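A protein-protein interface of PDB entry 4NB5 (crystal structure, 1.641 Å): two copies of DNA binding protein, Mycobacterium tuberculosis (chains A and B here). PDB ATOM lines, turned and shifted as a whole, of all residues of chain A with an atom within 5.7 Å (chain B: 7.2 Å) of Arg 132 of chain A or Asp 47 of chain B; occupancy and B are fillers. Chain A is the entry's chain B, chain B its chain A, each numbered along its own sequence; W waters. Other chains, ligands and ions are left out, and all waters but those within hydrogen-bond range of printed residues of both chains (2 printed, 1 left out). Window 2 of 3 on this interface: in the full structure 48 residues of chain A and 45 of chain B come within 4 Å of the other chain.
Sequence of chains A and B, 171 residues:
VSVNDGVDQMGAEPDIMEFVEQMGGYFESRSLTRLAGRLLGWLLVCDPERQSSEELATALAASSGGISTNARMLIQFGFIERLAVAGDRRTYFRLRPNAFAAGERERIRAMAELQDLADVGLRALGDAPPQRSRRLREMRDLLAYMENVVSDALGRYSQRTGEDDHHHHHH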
ATOM      1  N   LEU A 125     -15.728 -34.616   0.494  1.00  0.00           N
ATOM      2  CA  LEU A 125     -16.996 -34.000   0.099  1.00  0.00           C
ATOM      3  C   LEU A 125     -17.487 -34.513  -1.259  1.00  0.00           C
ATOM      4  O   LEU A 125     -18.359 -33.906  -1.876  1.00  0.00           O
ATOM      5  CB  LEU A 125     -16.871 -32.472   0.042  1.00  0.00           C
ATOM      6  CG  LEU A 125     -16.650 -31.721   1.362  1.00  0.00           C
ATOM      7  CD1 LEU A 125     -16.640 -30.210   1.133  1.00  0.00           C
ATOM      8  CD2 LEU A 125     -17.703 -32.113   2.389  1.00  0.00           C
ATOM      9  N   ALA A 128     -21.200 -34.746  -1.639  1.00  0.00           N
ATOM     10  CA  ALA A 128     -21.938 -33.537  -1.315  1.00  0.00           C
ATOM     11  C   ALA A 128     -22.223 -32.763  -2.590  1.00  0.00           C
ATOM     12  O   ALA A 128     -21.570 -32.991  -3.608  1.00  0.00           O
ATOM     13  CB  ALA A 128     -21.137 -32.667  -0.351  1.00  0.00           C
ATOM     14  N   PRO A 129     -23.183 -31.830  -2.536  1.00  0.00           N
ATOM     15  CA  PRO A 129     -23.425 -30.947  -3.676  1.00  0.00           C
ATOM     16  C   PRO A 129     -22.164 -30.168  -3.999  1.00  0.00           C
ATOM     17  O   PRO A 129     -21.452 -29.750  -3.082  1.00  0.00           O
ATOM     18  CB  PRO A 129     -24.514 -30.004  -3.172  1.00  0.00           C
ATOM     19  CG  PRO A 129     -25.133 -30.705  -2.031  1.00  0.00           C
ATOM     20  CD  PRO A 129     -24.064 -31.518  -1.402  1.00  0.00           C
ATOM     21  N   PRO A 130     -21.875 -29.977  -5.289  1.00  0.00           N
ATOM     22  CA  PRO A 130     -20.622 -29.295  -5.628  1.00  0.00           C
ATOM     23  C   PRO A 130     -20.499 -27.879  -5.047  1.00  0.00           C
ATOM     24  O   PRO A 130     -19.371 -27.425  -4.852  1.00  0.00           O
ATOM     25  CB  PRO A 130     -20.617 -29.277  -7.166  1.00  0.00           C
ATOM     26  CG  PRO A 130     -21.954 -29.768  -7.601  1.00  0.00           C
ATOM     27  CD  PRO A 130     -22.586 -30.494  -6.468  1.00  0.00           C
ATOM     28  N   GLN A 131     -21.610 -27.201  -4.765  1.00  0.00           N
ATOM     29  CA  GLN A 131     -21.560 -25.883  -4.132  1.00  0.00           C
ATOM     30  C   GLN A 131     -20.821 -25.927  -2.789  1.00  0.00           C
ATOM     31  O   GLN A 131     -20.149 -24.963  -2.402  1.00  0.00           O
ATOM     32  CB  GLN A 131     -22.968 -25.334  -3.891  1.00  0.00           C
ATOM     33  CG  GLN A 131     -23.735 -24.977  -5.161  1.00  0.00           C
ATOM     34  CD  GLN A 131     -24.645 -26.101  -5.608  1.00  0.00           C
ATOM     35  OE1 GLN A 131     -24.329 -27.275  -5.432  1.00  0.00           O
ATOM     36  NE2 GLN A 131     -25.795 -25.742  -6.174  1.00  0.00           N
ATOM     37  N   ARG A 132     -20.950 -27.041  -2.076  1.00  0.00           N
ATOM     38  CA  ARG A 132     -20.361 -27.152  -0.744  1.00  0.00           C
ATOM     39  C   ARG A 132     -18.839 -27.176  -0.828  1.00  0.00           C
ATOM     40  O   ARG A 132     -18.151 -26.793   0.124  1.00  0.00           O
ATOM     41  CB  ARG A 132     -20.853 -28.401  -0.023  1.00  0.00           C
ATOM     42  CG  ARG A 132     -20.505 -28.428   1.452  1.00  0.00           C
ATOM     43  CD  ARG A 132     -21.119 -29.613   2.177  1.00  0.00           C
ATOM     44  NE  ARG A 132     -20.450 -29.864   3.452  1.00  0.00           N
ATOM     45  CZ  ARG A 132     -20.581 -30.976   4.164  1.00  0.00           C
ATOM     46  NH1 ARG A 132     -21.391 -31.950   3.747  1.00  0.00           N
ATOM     47  NH2 ARG A 132     -19.909 -31.115   5.297  1.00  0.00           N
ATOM     48  N   SER A 133     -18.318 -27.626  -1.961  1.00  0.00           N
ATOM     49  CA  SER A 133     -16.869 -27.748  -2.165  1.00  0.00           C
ATOM     50  C   SER A 133     -16.216 -26.500  -2.760  1.00  0.00           C
ATOM     51  O   SER A 133     -15.002 -26.481  -2.974  1.00  0.00           O
ATOM     52  CB  SER A 133     -16.558 -28.947  -3.068  1.00  0.00           C
ATOM     53  OG  SER A 133     -16.599 -30.157  -2.347  1.00  0.00           O
ATOM     54  N   ARG A 134     -17.004 -25.459  -3.016  1.00  0.00           N
ATOM     55  CA  ARG A 134     -16.476 -24.240  -3.608  1.00  0.00           C
ATOM     56  C   ARG A 134     -15.306 -23.650  -2.811  1.00  0.00           C
ATOM     57  O   ARG A 134     -14.311 -23.235  -3.394  1.00  0.00           O
ATOM     58  CB  ARG A 134     -17.563 -23.183  -3.742  1.00  0.00           C
ATOM     59  CG  ARG A 134     -17.110 -21.951  -4.497  1.00  0.00           C
ATOM     60  CD  ARG A 134     -18.152 -20.845  -4.431  1.00  0.00           C
ATOM     61  NE  ARG A 134     -17.721 -19.640  -5.139  1.00  0.00           N
ATOM     62  CZ  ARG A 134     -18.376 -18.482  -5.122  1.00  0.00           C
ATOM     63  NH1 ARG A 134     -19.501 -18.353  -4.429  1.00  0.00           N
ATOM     64  NH2 ARG A 134     -17.902 -17.445  -5.800  1.00  0.00           N
ATOM     65  N   ARG A 135     -15.436 -23.591  -1.491  1.00  0.00           N
ATOM     66  CA  ARG A 135     -14.369 -23.032  -0.656  1.00  0.00           C
ATOM     67  C   ARG A 135     -13.049 -23.786  -0.826  1.00  0.00           C
ATOM     68  O   ARG A 135     -11.980 -23.174  -0.936  1.00  0.00           O
ATOM     69  CB  ARG A 135     -14.778 -23.057   0.818  1.00  0.00           C
ATOM     70  CG  ARG A 135     -15.899 -22.093   1.179  1.00  0.00           C
ATOM     71  CD  ARG A 135     -16.594 -22.557   2.453  1.00  0.00           C
ATOM     72  NE  ARG A 135     -17.401 -23.752   2.202  1.00  0.00           N
ATOM     73  CZ  ARG A 135     -17.976 -24.496   3.138  1.00  0.00           C
ATOM     74  NH1 ARG A 135     -17.841 -24.194   4.422  1.00  0.00           N
ATOM     75  NH2 ARG A 135     -18.697 -25.560   2.779  1.00  0.00           N
ATOM     76  N   LEU A 136     -13.117 -25.112  -0.841  1.00  0.00           N
ATOM     77  CA  LEU A 136     -11.916 -25.921  -1.005  1.00  0.00           C
ATOM     78  C   LEU A 136     -11.318 -25.758  -2.395  1.00  0.00           C
ATOM     79  O   LEU A 136     -10.094 -25.743  -2.544  1.00  0.00           O
ATOM     80  CB  LEU A 136     -12.210 -27.394  -0.751  1.00  0.00           C
ATOM     81  CG  LEU A 136     -12.326 -27.806   0.716  1.00  0.00           C
ATOM     82  CD1 LEU A 136     -12.962 -29.182   0.809  1.00  0.00           C
ATOM     83  CD2 LEU A 136     -10.978 -27.803   1.419  1.00  0.00           C
ATOM     84  N   ILE B  16     -14.848 -36.493   7.001  1.00  0.00           N
ATOM     85  CA  ILE B  16     -14.718 -35.047   7.109  1.00  0.00           C
ATOM     86  C   ILE B  16     -13.871 -34.736   8.333  1.00  0.00           C
ATOM     87  O   ILE B  16     -12.958 -33.910   8.271  1.00  0.00           O
ATOM     88  CB  ILE B  16     -16.083 -34.335   7.186  1.00  0.00           C
ATOM     89  CG1 ILE B  16     -16.563 -33.967   5.782  1.00  0.00           C
ATOM     90  CG2 ILE B  16     -16.001 -33.079   8.036  1.00  0.00           C
ATOM     91  CD1 ILE B  16     -15.613 -33.039   5.022  1.00  0.00           C
ATOM     92  N   TRP B  42     -12.763 -26.962   9.664  1.00  0.00           N
ATOM     93  CA  TRP B  42     -14.212 -27.047   9.801  1.00  0.00           C
ATOM     94  C   TRP B  42     -14.913 -25.981   8.954  1.00  0.00           C
ATOM     95  O   TRP B  42     -15.891 -26.266   8.274  1.00  0.00           O
ATOM     96  CB  TRP B  42     -14.628 -26.905  11.264  1.00  0.00           C
ATOM     97  CG  TRP B  42     -16.093 -27.073  11.470  1.00  0.00           C
ATOM     98  CD1 TRP B  42     -17.005 -26.094  11.734  1.00  0.00           C
ATOM     99  CD2 TRP B  42     -16.828 -28.295  11.391  1.00  0.00           C
ATOM    100  NE1 TRP B  42     -18.266 -26.634  11.824  1.00  0.00           N
ATOM    101  CE2 TRP B  42     -18.180 -27.990  11.633  1.00  0.00           C
ATOM    102  CE3 TRP B  42     -16.470 -29.630  11.161  1.00  0.00           C
ATOM    103  CZ2 TRP B  42     -19.181 -28.961  11.643  1.00  0.00           C
ATOM    104  CZ3 TRP B  42     -17.468 -30.597  11.174  1.00  0.00           C
ATOM    105  CH2 TRP B  42     -18.803 -30.255  11.413  1.00  0.00           C
ATOM    106  N   LEU B  44     -13.947 -24.628   6.321  1.00  0.00           N
ATOM    107  CA  LEU B  44     -13.749 -24.910   4.904  1.00  0.00           C
ATOM    108  C   LEU B  44     -14.761 -25.919   4.366  1.00  0.00           C
ATOM    109  O   LEU B  44     -15.018 -25.949   3.164  1.00  0.00           O
ATOM    110  CB  LEU B  44     -12.339 -25.436   4.655  1.00  0.00           C
ATOM    111  CG  LEU B  44     -11.292 -24.336   4.550  1.00  0.00           C
ATOM    112  CD1 LEU B  44      -9.897 -24.858   4.860  1.00  0.00           C
ATOM    113  CD2 LEU B  44     -11.334 -23.721   3.162  1.00  0.00           C
ATOM    114  N   VAL B  45     -15.328 -26.747   5.242  1.00  0.00           N
ATOM    115  CA  VAL B  45     -16.161 -27.860   4.776  1.00  0.00           C
ATOM    116  C   VAL B  45     -17.572 -27.907   5.352  1.00  0.00           C
ATOM    117  O   VAL B  45     -18.414 -28.680   4.876  1.00  0.00           O
ATOM    118  CB  VAL B  45     -15.489 -29.228   5.060  1.00  0.00           C
ATOM    119  CG1 VAL B  45     -14.161 -29.324   4.330  1.00  0.00           C
ATOM    120  CG2 VAL B  45     -15.312 -29.450   6.555  1.00  0.00           C
ATOM    121  N   CYS B  46     -17.847 -27.105   6.373  1.00  0.00           N
ATOM    122  CA  CYS B  46     -19.133 -27.188   7.062  1.00  0.00           C
ATOM    123  C   CYS B  46     -20.311 -26.711   6.208  1.00  0.00           C
ATOM    124  O   CYS B  46     -20.148 -25.937   5.265  1.00  0.00           O
ATOM    125  CB  CYS B  46     -19.083 -26.370   8.355  1.00  0.00           C
ATOM    126  SG  CYS B  46     -18.771 -24.616   8.114  1.00  0.00           S
ATOM    127  N   ASP B  47     -21.513 -27.164   6.558  1.00  0.00           N
ATOM    128  CA  ASP B  47     -22.721 -26.695   5.901  1.00  0.00           C
ATOM    129  C   ASP B  47     -23.798 -26.509   6.964  1.00  0.00           C
ATOM    130  O   ASP B  47     -24.037 -27.422   7.755  1.00  0.00           O
ATOM    131  CB  ASP B  47     -23.178 -27.711   4.848  1.00  0.00           C
ATOM    132  CG  ASP B  47     -24.400 -27.243   4.069  1.00  0.00           C
ATOM    133  OD1 ASP B  47     -24.362 -26.155   3.455  1.00  0.00           O
ATOM    134  OD2 ASP B  47     -25.405 -27.977   4.068  1.00  0.00           O
ATOM    135  N   PRO B  48     -24.402 -25.314   7.039  1.00  0.00           N
ATOM    136  CA  PRO B  48     -24.175 -24.078   6.282  1.00  0.00           C
ATOM    137  C   PRO B  48     -22.754 -23.556   6.477  1.00  0.00           C
ATOM    138  O   PRO B  48     -22.082 -23.976   7.412  1.00  0.00           O
ATOM    139  CB  PRO B  48     -25.156 -23.087   6.925  1.00  0.00           C
ATOM    140  CG  PRO B  48     -26.158 -23.906   7.611  1.00  0.00           C
ATOM    141  CD  PRO B  48     -25.479 -25.156   8.032  1.00  0.00           C
ATOM    142  N   GLU B  49     -22.322 -22.641   5.625  1.00  0.00           N
ATOM    143  CA  GLU B  49     -20.991 -22.054   5.772  1.00  0.00           C
ATOM    144  C   GLU B  49     -20.864 -21.310   7.094  1.00  0.00           C
ATOM    145  O   GLU B  49     -19.825 -21.376   7.748  1.00  0.00           O
ATOM    146  CB  GLU B  49     -20.690 -21.136   4.592  1.00  0.00           C
ATOM    147  CG  GLU B  49     -20.616 -21.907   3.288  1.00  0.00           C
ATOM    148  CD  GLU B  49     -20.155 -21.072   2.114  1.00  0.00           C
ATOM    149  OE1 GLU B  49     -19.639 -19.952   2.321  1.00  0.00           O
ATOM    150  OE2 GLU B  49     -20.305 -21.554   0.968  1.00  0.00           O
ATOM    151  N   ARG B  50     -21.923 -20.617   7.503  1.00  0.00           N
ATOM    152  CA  ARG B  50     -21.897 -19.895   8.765  1.00  0.00           C
ATOM    153  C   ARG B  50     -22.137 -20.853   9.925  1.00  0.00           C
ATOM    154  O   ARG B  50     -22.908 -21.806   9.807  1.00  0.00           O
ATOM    155  CB  ARG B  50     -22.902 -18.743   8.780  1.00  0.00           C
ATOM    156  CG  ARG B  50     -24.353 -19.191   8.927  1.00  0.00           C
ATOM    157  CD  ARG B  50     -25.304 -18.039   8.673  1.00  0.00           C
ATOM    158  NE  ARG B  50     -26.684 -18.446   8.934  1.00  0.00           N
ATOM    159  CZ  ARG B  50     -27.753 -17.804   8.478  1.00  0.00           C
ATOM    160  NH1 ARG B  50     -27.616 -16.723   7.724  1.00  0.00           N
ATOM    161  NH2 ARG B  50     -28.963 -18.251   8.772  1.00  0.00           N
ATOM    162  N   GLN B  51     -21.442 -20.599  11.031  1.00  0.00           N
ATOM    163  CA  GLN B  51     -21.517 -21.437  12.222  1.00  0.00           C
ATOM    164  C   GLN B  51     -21.540 -20.545  13.448  1.00  0.00           C
ATOM    165  O   GLN B  51     -20.748 -19.612  13.565  1.00  0.00           O
ATOM    166  CB  GLN B  51     -20.302 -22.363  12.307  1.00  0.00           C
ATOM    167  CG  GLN B  51     -20.166 -23.314  11.130  1.00  0.00           C
ATOM    168  CD  GLN B  51     -21.030 -24.541  11.274  1.00  0.00           C
ATOM    169  OE1 GLN B  51     -20.850 -25.339  12.193  1.00  0.00           O
ATOM    170  NE2 GLN B  51     -21.980 -24.708  10.356  1.00  0.00           N
HETATM  171  O   HOH W   1     -15.483 -26.397   0.535  1.00  0.00           O
HETATM  172  O   HOH W   2     -22.023 -25.266   3.049  1.00  0.00           O
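No position is printed for both chains. Of the 8 pairs that touch across the chains among the printed residues, none has its exchanged pair printed and touching as well.
O of Leu 44 of chain B lies close to NE of Arg 135 of chain A, 3.4 Å away. The guanidinium group (NH2) of Arg 135 of chain A sits at hydrogen-bond distance from the backbone carbonyl oxygen (O) of Cys 46 of chain B (2.9 Å). OE2 of Glu 49 of chain B is in salt-bridge range of NE of Arg 135 of chain A, 3.8 Å away. O of Val 45 of chain B is in hydrogen-bond range of NE of Arg 132 of chain A (2.8 Å).
Water W2 lies within hydrogen-bond range of OD1 of Asp 47 of chain B (2.5 Å), O of Cys 46 of chain B (3.0 Å) and NH2 of Arg 135 of chain A (3.3 Å). Water W1 lies within hydrogen-bond range of O of Leu 44 of chain B (2.7 Å), O of Arg 132 of chain A (2.7 Å), N of Leu 136 of chain A (3.0 Å) and N of Arg 135 of chain A (3.5 Å).
Among the printed residues, pairs that only touch across the chains: Leu 125 of chain A with Ile 16 of chain B (3.5 Å), Arg 135 of chain A with Val 45 of chain B (3.7 Å), Leu 136 of chain A with Val 45 of chain B (3.7 Å) and Arg 132 of chain A with Asp 47 of chain B (3.7 Å).
O of Trp 42 of chain B lies close to SG of Cys 46 of chain B (3.3 Å). The side-chain sulfur of Cys 46 of chain B sits at hydrogen-bond distance from the backbone carbonyl oxygen of Pro 48 of chain B (3.4 Å). SG of Cys 46 of chain B sits at hydrogen-bond distance from O of Glu 49 of chain B, 3.4 Å away. The guanidinium group (NH2) of Arg 135 of chain A lies within hydrogen-bond range of the backbone carbonyl oxygen (O) of Arg 132 of chain A, at 3.0 Å.
Hydrophobic or aromatic side chains of chain A that line the printed part of chain B: Leu 125 and Leu 136. Of the 10 printed residues of chain B, 6 touch a printed residue of chain A. Hydrophobic or aromatic side chains of chain B within 4 Å of the printed part of chain A: Ile 16 and Val 45.
Of chain B, only Val 45 and Asp 47 come within 4 Å of Arg 132 of chain A. Of the printed residues of chain A, Asp 47 of chain B touches Arg 132. Of the printed residues of chain A, Cys 46 of chain B touches Arg 135. Printed residues of chain B within 4 Å of Leu 125 of chain A: Ile 16 (3.5 Å). Printed residues of chain A within 4 Å of Ile 16 of chain B: Leu 125. The nearest residue of chain B that does not touch Arg 132 of chain A is Cys 46 of chain B (4.2 Å). The nearest residue of chain A that does not touch Asp 47 of chain B is Arg 135 of chain A (5.0 Å).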
